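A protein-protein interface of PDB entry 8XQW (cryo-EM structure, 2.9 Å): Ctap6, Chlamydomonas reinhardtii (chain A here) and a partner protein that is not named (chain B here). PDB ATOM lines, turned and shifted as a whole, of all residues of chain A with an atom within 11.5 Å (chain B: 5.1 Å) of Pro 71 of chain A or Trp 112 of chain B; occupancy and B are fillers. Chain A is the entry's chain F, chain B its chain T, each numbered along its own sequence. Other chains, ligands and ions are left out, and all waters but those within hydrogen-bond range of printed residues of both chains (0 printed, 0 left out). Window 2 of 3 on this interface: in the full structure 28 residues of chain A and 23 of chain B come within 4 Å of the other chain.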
ATOM      1  N   PRO A  68      -2.232 -21.773  -4.496  1.00  0.00           N
ATOM      2  CA  PRO A  68      -0.798 -21.756  -4.803  1.00  0.00           C
ATOM      3  C   PRO A  68       0.063 -21.581  -3.554  1.00  0.00           C
ATOM      4  O   PRO A  68       0.021 -20.538  -2.903  1.00  0.00           O
ATOM      5  CB  PRO A  68      -0.655 -20.559  -5.746  1.00  0.00           C
ATOM      6  CG  PRO A  68      -1.796 -19.672  -5.406  1.00  0.00           C
ATOM      7  CD  PRO A  68      -2.920 -20.562  -4.972  1.00  0.00           C
ATOM      8  N   ALA A  69       0.835 -22.611  -3.223  1.00  0.00           N
ATOM      9  CA  ALA A  69       1.661 -22.571  -2.027  1.00  0.00           C
ATOM     10  C   ALA A  69       2.864 -21.661  -2.230  1.00  0.00           C
ATOM     11  O   ALA A  69       3.514 -21.687  -3.278  1.00  0.00           O
ATOM     12  CB  ALA A  69       2.128 -23.977  -1.657  1.00  0.00           C
ATOM     13  N   LEU A  70       3.155 -20.853  -1.215  1.00  0.00           N
ATOM     14  CA  LEU A  70       4.358 -20.041  -1.226  1.00  0.00           C
ATOM     15  C   LEU A  70       5.582 -20.949  -1.311  1.00  0.00           C
ATOM     16  O   LEU A  70       5.524 -22.114  -0.911  1.00  0.00           O
ATOM     17  CB  LEU A  70       4.443 -19.182   0.036  1.00  0.00           C
ATOM     18  CG  LEU A  70       3.844 -17.777   0.013  1.00  0.00           C
ATOM     19  CD1 LEU A  70       4.435 -16.945  -1.107  1.00  0.00           C
ATOM     20  CD2 LEU A  70       2.342 -17.863  -0.130  1.00  0.00           C
ATOM     21  N   PRO A  71       6.698 -20.454  -1.839  1.00  0.00           N
ATOM     22  CA  PRO A  71       7.925 -21.247  -1.801  1.00  0.00           C
ATOM     23  C   PRO A  71       8.396 -21.427  -0.367  1.00  0.00           C
ATOM     24  O   PRO A  71       8.052 -20.657   0.531  1.00  0.00           O
ATOM     25  CB  PRO A  71       8.915 -20.418  -2.626  1.00  0.00           C
ATOM     26  CG  PRO A  71       8.385 -19.039  -2.580  1.00  0.00           C
ATOM     27  CD  PRO A  71       6.895 -19.170  -2.532  1.00  0.00           C
ATOM     28  N   ALA A  72       9.178 -22.478  -0.157  1.00  0.00           N
ATOM     29  CA  ALA A  72       9.670 -22.767   1.178  1.00  0.00           C
ATOM     30  C   ALA A  72      10.575 -21.644   1.663  1.00  0.00           C
ATOM     31  O   ALA A  72      11.139 -20.886   0.872  1.00  0.00           O
ATOM     32  CB  ALA A  72      10.422 -24.099   1.194  1.00  0.00           C
ATOM     33  N   ARG A  73      10.697 -21.529   2.985  1.00  0.00           N
ATOM     34  CA  ARG A  73      11.597 -20.539   3.576  1.00  0.00           C
ATOM     35  C   ARG A  73      12.071 -21.096   4.914  1.00  0.00           C
ATOM     36  O   ARG A  73      11.369 -20.977   5.922  1.00  0.00           O
ATOM     37  CB  ARG A  73      10.914 -19.191   3.740  1.00  0.00           C
ATOM     38  CG  ARG A  73      11.764 -18.149   4.445  1.00  0.00           C
ATOM     39  CD  ARG A  73      11.131 -16.770   4.342  1.00  0.00           C
ATOM     40  NE  ARG A  73       9.694 -16.813   4.600  1.00  0.00           N
ATOM     41  CZ  ARG A  73       9.146 -16.678   5.803  1.00  0.00           C
ATOM     42  NH1 ARG A  73       9.915 -16.484   6.865  1.00  0.00           N
ATOM     43  NH2 ARG A  73       7.830 -16.734   5.945  1.00  0.00           N
ATOM     44  N   ALA A  74      13.251 -21.698   4.912  1.00  0.00           N
ATOM     45  CA  ALA A  74      13.884 -22.209   6.117  1.00  0.00           C
ATOM     46  C   ALA A  74      15.142 -21.399   6.413  1.00  0.00           C
ATOM     47  O   ALA A  74      15.673 -20.693   5.555  1.00  0.00           O
ATOM     48  CB  ALA A  74      14.207 -23.699   5.976  1.00  0.00           C
ATOM     49  N   THR A  75      15.622 -21.511   7.645  1.00  0.00           N
ATOM     50  CA  THR A  75      16.793 -20.762   8.067  1.00  0.00           C
ATOM     51  C   THR A  75      17.492 -21.543   9.170  1.00  0.00           C
ATOM     52  O   THR A  75      16.847 -22.068  10.079  1.00  0.00           O
ATOM     53  CB  THR A  75      16.416 -19.358   8.550  1.00  0.00           C
ATOM     54  OG1 THR A  75      15.917 -18.597   7.445  1.00  0.00           O
ATOM     55  CG2 THR A  75      17.624 -18.646   9.128  1.00  0.00           C
ATOM     56  N   TYR A  98      22.180 -25.446  -4.311  1.00  0.00           N
ATOM     57  CA  TYR A  98      21.541 -24.463  -5.170  1.00  0.00           C
ATOM     58  C   TYR A  98      22.092 -23.081  -4.848  1.00  0.00           C
ATOM     59  O   TYR A  98      22.783 -22.883  -3.847  1.00  0.00           O
ATOM     60  CB  TYR A  98      20.017 -24.494  -5.004  1.00  0.00           C
ATOM     61  CG  TYR A  98      19.408 -25.859  -5.231  1.00  0.00           C
ATOM     62  CD1 TYR A  98      19.552 -26.871  -4.296  1.00  0.00           C
ATOM     63  CD2 TYR A  98      18.688 -26.134  -6.378  1.00  0.00           C
ATOM     64  CE1 TYR A  98      19.011 -28.110  -4.502  1.00  0.00           C
ATOM     65  CE2 TYR A  98      18.136 -27.375  -6.588  1.00  0.00           C
ATOM     66  CZ  TYR A  98      18.301 -28.358  -5.648  1.00  0.00           C
ATOM     67  OH  TYR A  98      17.753 -29.600  -5.854  1.00  0.00           O
ATOM     68  N   ASP A  99      21.787 -22.118  -5.704  1.00  0.00           N
ATOM     69  CA  ASP A  99      22.369 -20.789  -5.593  1.00  0.00           C
ATOM     70  C   ASP A  99      21.325 -19.781  -5.126  1.00  0.00           C
ATOM     71  O   ASP A  99      20.156 -20.100  -4.916  1.00  0.00           O
ATOM     72  CB  ASP A  99      22.996 -20.365  -6.921  1.00  0.00           C
ATOM     73  CG  ASP A  99      21.996 -19.748  -7.864  1.00  0.00           C
ATOM     74  OD1 ASP A  99      21.717 -18.535  -7.741  1.00  0.00           O
ATOM     75  OD2 ASP A  99      21.489 -20.478  -8.737  1.00  0.00           O
ATOM     76  N   ASN A 100      21.769 -18.536  -4.973  1.00  0.00           N
ATOM     77  CA  ASN A 100      20.934 -17.509  -4.364  1.00  0.00           C
ATOM     78  C   ASN A 100      19.963 -16.897  -5.366  1.00  0.00           C
ATOM     79  O   ASN A 100      18.744 -16.959  -5.179  1.00  0.00           O
ATOM     80  CB  ASN A 100      21.819 -16.424  -3.756  1.00  0.00           C
ATOM     81  CG  ASN A 100      22.839 -16.982  -2.811  1.00  0.00           C
ATOM     82  OD1 ASN A 100      22.506 -17.743  -1.905  1.00  0.00           O
ATOM     83  ND2 ASN A 100      24.097 -16.624  -3.018  1.00  0.00           N
ATOM     84  N   VAL A 101      20.487 -16.286  -6.429  1.00  0.00           N
ATOM     85  CA  VAL A 101      19.636 -15.539  -7.348  1.00  0.00           C
ATOM     86  C   VAL A 101      18.678 -16.473  -8.066  1.00  0.00           C
ATOM     87  O   VAL A 101      17.455 -16.325  -7.973  1.00  0.00           O
ATOM     88  CB  VAL A 101      20.492 -14.744  -8.344  1.00  0.00           C
ATOM     89  CG1 VAL A 101      19.603 -13.983  -9.288  1.00  0.00           C
ATOM     90  CG2 VAL A 101      21.407 -13.808  -7.603  1.00  0.00           C
ATOM     91  N   TYR A 102      19.212 -17.444  -8.789  1.00  0.00           N
ATOM     92  CA  TYR A 102      18.409 -18.479  -9.412  1.00  0.00           C
ATOM     93  C   TYR A 102      18.295 -19.664  -8.467  1.00  0.00           C
ATOM     94  O   TYR A 102      19.089 -19.834  -7.540  1.00  0.00           O
ATOM     95  CB  TYR A 102      19.023 -18.931 -10.738  1.00  0.00           C
ATOM     96  CG  TYR A 102      19.234 -17.832 -11.752  1.00  0.00           C
ATOM     97  CD1 TYR A 102      20.374 -17.042 -11.727  1.00  0.00           C
ATOM     98  CD2 TYR A 102      18.304 -17.597 -12.745  1.00  0.00           C
ATOM     99  CE1 TYR A 102      20.568 -16.043 -12.655  1.00  0.00           C
ATOM    100  CE2 TYR A 102      18.492 -16.602 -13.673  1.00  0.00           C
ATOM    101  CZ  TYR A 102      19.621 -15.830 -13.624  1.00  0.00           C
ATOM    102  OH  TYR A 102      19.804 -14.837 -14.554  1.00  0.00           O
ATOM    103  N   GLY A 103      17.273 -20.473  -8.689  1.00  0.00           N
ATOM    104  CA  GLY A 103      17.165 -21.722  -7.970  1.00  0.00           C
ATOM    105  C   GLY A 103      17.730 -22.874  -8.767  1.00  0.00           C
ATOM    106  O   GLY A 103      17.007 -23.820  -9.082  1.00  0.00           O
ATOM    107  N   LEU A 104      19.001 -22.813  -9.112  1.00  0.00           N
ATOM    108  CA  LEU A 104      19.494 -23.868  -9.975  1.00  0.00           C
ATOM    109  C   LEU A 104      20.640 -24.627  -9.321  1.00  0.00           C
ATOM    110  O   LEU A 104      21.376 -24.071  -8.503  1.00  0.00           O
ATOM    111  CB  LEU A 104      19.965 -23.296 -11.313  1.00  0.00           C
ATOM    112  CG  LEU A 104      18.915 -22.446 -12.016  1.00  0.00           C
ATOM    113  CD1 LEU A 104      19.459 -21.897 -13.303  1.00  0.00           C
ATOM    114  CD2 LEU A 104      17.689 -23.276 -12.282  1.00  0.00           C
ATOM    115  N   VAL A 223       6.656  -3.422  -8.444  1.00  0.00           N
ATOM    116  CA  VAL A 223       6.134  -4.686  -8.951  1.00  0.00           C
ATOM    117  C   VAL A 223       4.610  -4.682  -8.962  1.00  0.00           C
ATOM    118  O   VAL A 223       3.985  -5.139  -9.926  1.00  0.00           O
ATOM    119  CB  VAL A 223       6.693  -5.860  -8.129  1.00  0.00           C
ATOM    120  CG1 VAL A 223       8.051  -6.272  -8.662  1.00  0.00           C
ATOM    121  CG2 VAL A 223       6.798  -5.473  -6.664  1.00  0.00           C
ATOM    122  N   GLU A 237      -1.976  -5.596  -9.303  1.00  0.00           N
ATOM    123  CA  GLU A 237      -0.942  -5.748 -10.310  1.00  0.00           C
ATOM    124  C   GLU A 237      -0.965  -4.549 -11.254  1.00  0.00           C
ATOM    125  O   GLU A 237      -1.955  -3.825 -11.364  1.00  0.00           O
ATOM    126  CB  GLU A 237      -1.129  -7.052 -11.081  1.00  0.00           C
ATOM    127  CG  GLU A 237      -1.358  -8.276 -10.208  1.00  0.00           C
ATOM    128  CD  GLU A 237      -0.069  -8.895  -9.700  1.00  0.00           C
ATOM    129  OE1 GLU A 237       0.972  -8.208  -9.704  1.00  0.00           O
ATOM    130  OE2 GLU A 237      -0.096 -10.080  -9.302  1.00  0.00           O
ATOM    131  N   ARG A 244       4.820  -7.716 -16.130  1.00  0.00           N
ATOM    132  CA  ARG A 244       5.919  -8.528 -16.642  1.00  0.00           C
ATOM    133  C   ARG A 244       5.589 -10.015 -16.560  1.00  0.00           C
ATOM    134  O   ARG A 244       5.444 -10.685 -17.585  1.00  0.00           O
ATOM    135  CB  ARG A 244       7.207  -8.213 -15.878  1.00  0.00           C
ATOM    136  CG  ARG A 244       7.678  -6.774 -16.021  1.00  0.00           C
ATOM    137  CD  ARG A 244       8.342  -6.536 -17.366  1.00  0.00           C
ATOM    138  NE  ARG A 244       9.196  -7.651 -17.750  1.00  0.00           N
ATOM    139  CZ  ARG A 244       9.752  -7.788 -18.948  1.00  0.00           C
ATOM    140  NH1 ARG A 244       9.548  -6.875 -19.886  1.00  0.00           N
ATOM    141  NH2 ARG A 244      10.509  -8.842 -19.209  1.00  0.00           N
ATOM    142  N   GLY A 245       5.422 -10.536 -15.351  1.00  0.00           N
ATOM    143  CA  GLY A 245       5.384 -11.977 -15.192  1.00  0.00           C
ATOM    144  C   GLY A 245       4.087 -12.654 -15.575  1.00  0.00           C
ATOM    145  O   GLY A 245       4.040 -13.380 -16.572  1.00  0.00           O
ATOM    146  N   ALA A 246       3.027 -12.400 -14.810  1.00  0.00           N
ATOM    147  CA  ALA A 246       1.741 -13.059 -15.005  1.00  0.00           C
ATOM    148  C   ALA A 246       0.713 -12.488 -14.039  1.00  0.00           C
ATOM    149  O   ALA A 246       1.065 -11.730 -13.130  1.00  0.00           O
ATOM    150  CB  ALA A 246       1.858 -14.571 -14.804  1.00  0.00           C
ATOM    151  N   ALA A 247      -0.554 -12.857 -14.214  1.00  0.00           N
ATOM    152  CA  ALA A 247      -1.627 -12.377 -13.344  1.00  0.00           C
ATOM    153  C   ALA A 247      -1.591 -13.185 -12.056  1.00  0.00           C
ATOM    154  O   ALA A 247      -2.319 -14.162 -11.888  1.00  0.00           O
ATOM    155  CB  ALA A 247      -2.976 -12.486 -14.040  1.00  0.00           C
ATOM    156  N   VAL A 248      -0.726 -12.771 -11.127  1.00  0.00           N
ATOM    157  CA  VAL A 248      -0.602 -13.462  -9.847  1.00  0.00           C
ATOM    158  C   VAL A 248      -1.584 -12.953  -8.807  1.00  0.00           C
ATOM    159  O   VAL A 248      -2.286 -13.767  -8.187  1.00  0.00           O
ATOM    160  CB  VAL A 248       0.836 -13.363  -9.295  1.00  0.00           C
ATOM    161  CG1 VAL A 248       0.873 -13.735  -7.819  1.00  0.00           C
ATOM    162  CG2 VAL A 248       1.759 -14.272 -10.083  1.00  0.00           C
ATOM    163  N   GLY A 249      -1.675 -11.644  -8.605  1.00  0.00           N
ATOM    164  CA  GLY A 249      -2.534 -11.101  -7.585  1.00  0.00           C
ATOM    165  C   GLY A 249      -3.851 -10.619  -8.145  1.00  0.00           C
ATOM    166  O   GLY A 249      -4.393 -11.182  -9.099  1.00  0.00           O
ATOM    167  N   PRO B 107       9.347  -9.550  -3.369  1.00  0.00           N
ATOM    168  CA  PRO B 107       9.650  -9.531  -4.812  1.00  0.00           C
ATOM    169  C   PRO B 107      10.176 -10.854  -5.345  1.00  0.00           C
ATOM    170  O   PRO B 107       9.680 -11.361  -6.364  1.00  0.00           O
ATOM    171  CB  PRO B 107      10.690  -8.412  -4.924  1.00  0.00           C
ATOM    172  CG  PRO B 107      10.341  -7.485  -3.809  1.00  0.00           C
ATOM    173  CD  PRO B 107       9.852  -8.350  -2.682  1.00  0.00           C
ATOM    174  N   GLU B 108      11.166 -11.434  -4.668  1.00  0.00           N
ATOM    175  CA  GLU B 108      11.748 -12.678  -5.147  1.00  0.00           C
ATOM    176  C   GLU B 108      10.713 -13.791  -5.220  1.00  0.00           C
ATOM    177  O   GLU B 108      10.619 -14.480  -6.242  1.00  0.00           O
ATOM    178  CB  GLU B 108      12.916 -13.095  -4.254  1.00  0.00           C
ATOM    179  CG  GLU B 108      12.662 -12.942  -2.760  1.00  0.00           C
ATOM    180  CD  GLU B 108      12.950 -11.543  -2.251  1.00  0.00           C
ATOM    181  OE1 GLU B 108      13.326 -10.681  -3.070  1.00  0.00           O
ATOM    182  OE2 GLU B 108      12.799 -11.305  -1.037  1.00  0.00           O
ATOM    183  N   GLU B 109       9.903 -13.969  -4.176  1.00  0.00           N
ATOM    184  CA  GLU B 109       8.949 -15.068  -4.216  1.00  0.00           C
ATOM    185  C   GLU B 109       7.798 -14.789  -5.173  1.00  0.00           C
ATOM    186  O   GLU B 109       7.246 -15.728  -5.753  1.00  0.00           O
ATOM    187  CB  GLU B 109       8.417 -15.391  -2.823  1.00  0.00           C
ATOM    188  CG  GLU B 109       7.440 -14.396  -2.245  1.00  0.00           C
ATOM    189  CD  GLU B 109       7.522 -14.361  -0.741  1.00  0.00           C
ATOM    190  OE1 GLU B 109       8.042 -15.335  -0.162  1.00  0.00           O
ATOM    191  OE2 GLU B 109       7.076 -13.372  -0.130  1.00  0.00           O
ATOM    192  N   LEU B 110       7.399 -13.529  -5.349  1.00  0.00           N
ATOM    193  CA  LEU B 110       6.345 -13.274  -6.321  1.00  0.00           C
ATOM    194  C   LEU B 110       6.832 -13.626  -7.720  1.00  0.00           C
ATOM    195  O   LEU B 110       6.100 -14.235  -8.512  1.00  0.00           O
ATOM    196  CB  LEU B 110       5.857 -11.824  -6.247  1.00  0.00           C
ATOM    197  CG  LEU B 110       6.731 -10.590  -6.454  1.00  0.00           C
ATOM    198  CD1 LEU B 110       6.994 -10.321  -7.924  1.00  0.00           C
ATOM    199  CD2 LEU B 110       6.092  -9.376  -5.809  1.00  0.00           C
ATOM    200  N   THR B 111       8.090 -13.294  -8.028  1.00  0.00           N
ATOM    201  CA  THR B 111       8.667 -13.748  -9.288  1.00  0.00           C
ATOM    202  C   THR B 111       8.744 -15.265  -9.326  1.00  0.00           C
ATOM    203  O   THR B 111       8.595 -15.882 -10.387  1.00  0.00           O
ATOM    204  CB  THR B 111      10.050 -13.138  -9.484  1.00  0.00           C
ATOM    205  OG1 THR B 111      10.809 -13.297  -8.282  1.00  0.00           O
ATOM    206  CG2 THR B 111       9.931 -11.663  -9.805  1.00  0.00           C
ATOM    207  N   TRP B 112       8.981 -15.882  -8.170  1.00  0.00           N
ATOM    208  CA  TRP B 112       9.000 -17.336  -8.083  1.00  0.00           C
ATOM    209  C   TRP B 112       7.677 -17.928  -8.548  1.00  0.00           C
ATOM    210  O   TRP B 112       7.650 -18.822  -9.399  1.00  0.00           O
ATOM    211  CB  TRP B 112       9.310 -17.756  -6.651  1.00  0.00           C
ATOM    212  CG  TRP B 112       9.648 -19.187  -6.497  1.00  0.00           C
ATOM    213  CD1 TRP B 112      10.890 -19.740  -6.532  1.00  0.00           C
ATOM    214  CD2 TRP B 112       8.734 -20.263  -6.265  1.00  0.00           C
ATOM    215  NE1 TRP B 112      10.809 -21.096  -6.344  1.00  0.00           N
ATOM    216  CE2 TRP B 112       9.494 -21.442  -6.176  1.00  0.00           C
ATOM    217  CE3 TRP B 112       7.346 -20.342  -6.126  1.00  0.00           C
ATOM    218  CZ2 TRP B 112       8.915 -22.684  -5.957  1.00  0.00           C
ATOM    219  CZ3 TRP B 112       6.775 -21.578  -5.908  1.00  0.00           C
ATOM    220  CH2 TRP B 112       7.557 -22.731  -5.825  1.00  0.00           C
ATOM    221  N   LEU B 113       6.564 -17.426  -8.019  1.00  0.00           N
ATOM    222  CA  LEU B 113       5.269 -17.951  -8.451  1.00  0.00           C
ATOM    223  C   LEU B 113       4.939 -17.553  -9.886  1.00  0.00           C
ATOM    224  O   LEU B 113       4.230 -18.285 -10.584  1.00  0.00           O
ATOM    225  CB  LEU B 113       4.143 -17.536  -7.500  1.00  0.00           C
ATOM    226  CG  LEU B 113       4.097 -18.103  -6.073  1.00  0.00           C
ATOM    227  CD1 LEU B 113       4.844 -17.284  -5.055  1.00  0.00           C
ATOM    228  CD2 LEU B 113       2.655 -18.273  -5.640  1.00  0.00           C
ATOM    229  N   LYS B 114       5.441 -16.410 -10.360  1.00  0.00           N
ATOM    230  CA  LYS B 114       5.237 -16.084 -11.771  1.00  0.00           C
ATOM    231  C   LYS B 114       5.899 -17.119 -12.674  1.00  0.00           C
ATOM    232  O   LYS B 114       5.283 -17.612 -13.633  1.00  0.00           O
ATOM    233  CB  LYS B 114       5.776 -14.691 -12.076  1.00  0.00           C
ATOM    234  CG  LYS B 114       4.997 -13.573 -11.431  1.00  0.00           C
ATOM    235  CD  LYS B 114       5.721 -12.259 -11.574  1.00  0.00           C
ATOM    236  CE  LYS B 114       4.756 -11.100 -11.448  1.00  0.00           C
ATOM    237  NZ  LYS B 114       5.288  -9.854 -12.068  1.00  0.00           N
ATOM    238  N   MET B 115       7.151 -17.466 -12.378  1.00  0.00           N
ATOM    239  CA  MET B 115       7.840 -18.487 -13.156  1.00  0.00           C
ATOM    240  C   MET B 115       7.180 -19.847 -12.984  1.00  0.00           C
ATOM    241  O   MET B 115       7.144 -20.654 -13.921  1.00  0.00           O
ATOM    242  CB  MET B 115       9.313 -18.546 -12.757  1.00  0.00           C
ATOM    243  CG  MET B 115      10.258 -18.856 -13.908  1.00  0.00           C
ATOM    244  SD  MET B 115      10.095 -17.767 -15.339  1.00  0.00           S
ATOM    245  CE  MET B 115      10.144 -16.149 -14.574  1.00  0.00           C
ATOM    246  N   ARG B 116       6.654 -20.121 -11.788  1.00  0.00           N
ATOM    247  CA  ARG B 116       5.903 -21.352 -11.573  1.00  0.00           C
ATOM    248  C   ARG B 116       4.713 -21.430 -12.515  1.00  0.00           C
ATOM    249  O   ARG B 116       4.504 -22.449 -13.184  1.00  0.00           O
ATOM    250  CB  ARG B 116       5.442 -21.426 -10.119  1.00  0.00           C
ATOM    251  CG  ARG B 116       4.634 -22.655  -9.782  1.00  0.00           C
ATOM    252  CD  ARG B 116       5.317 -23.465  -8.697  1.00  0.00           C
ATOM    253  NE  ARG B 116       4.545 -24.645  -8.332  1.00  0.00           N
ATOM    254  CZ  ARG B 116       3.520 -24.635  -7.485  1.00  0.00           C
ATOM    255  NH1 ARG B 116       3.139 -23.501  -6.911  1.00  0.00           N
ATOM    256  NH2 ARG B 116       2.875 -25.760  -7.212  1.00  0.00           N
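Ala 69 of chain A touches none of the printed residues of chain B.
Printed residues of chain B within 4 Å of Leu 70 of chain A: Leu 113 (3.98 Å).
Pro 71 of chain A touches three residues of chain B.
Ala 72 of chain A touches none of the printed residues of chain B.
Of the printed residues of chain B, Ala 246 of chain A touches Lys 114 (3.998 Å).
Of chain A, only Pro 71 (3.7 Å) comes within 4 Å of Glu 109 of chain B.
No residue of chain A comes within 4 Å of Thr 111 of chain B.
No residue of chain A comes within 4 Å of Met 115 of chain B.
No residue of chain A comes within 4 Å of Arg 116 of chain B.
The nearest printed residue of chain B that does not touch Pro 71 of chain A is Leu 110 of chain B (6.2 Å).
The nearest residue of chain A that does not touch Trp 112 of chain B is Ala 69 of chain A (4.2 Å).
Among the printed residues, pairs that only touch across the chains: Leu 70 of chain A with Leu 113 of chain B (3.98 Å), Pro 71 of chain A with Glu 109 of chain B (3.7 Å), Pro 71 of chain A with Trp 112 of chain B (3.6 Å), Pro 71 of chain A with Leu 113 of chain B (3.8 Å), Ala 246 of chain A with Lys 114 of chain B (3.998 Å) and Val 248 of chain A with Lys 114 of chain B (3.6 Å).
Of the 23 printed residues of chain A, 5 touch a printed residue of chain B.
Hydrophobic or aromatic side chains of chain A that line the printed part of chain B: Leu 70, Pro 71 and Val 248.
Of the 10 printed residues of chain B, 4 touch a printed residue of chain A.
Printed residues of chain B that touch a printed residue of chain A: Glu 109, Trp 112, Leu 113 and Lys 114.
Hydrophobic or aromatic side chains of chain B that line the printed part of chain A: Trp 112 and Leu 113.
Among the printed residues, no Asp or Glu carboxylate lies within 4 Å of a Lys or Arg side-chain nitrogen of the other chain.
The backbone NH (N) of Gly 245 of chain A lies close to the side-chain amino group (NZ) of Lys 114 of chain B.
The side-chain carboxylate (OE2) of Glu 237 of chain A lies close to the backbone NH (N) of Val 248 of chain A (3.3 Å).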
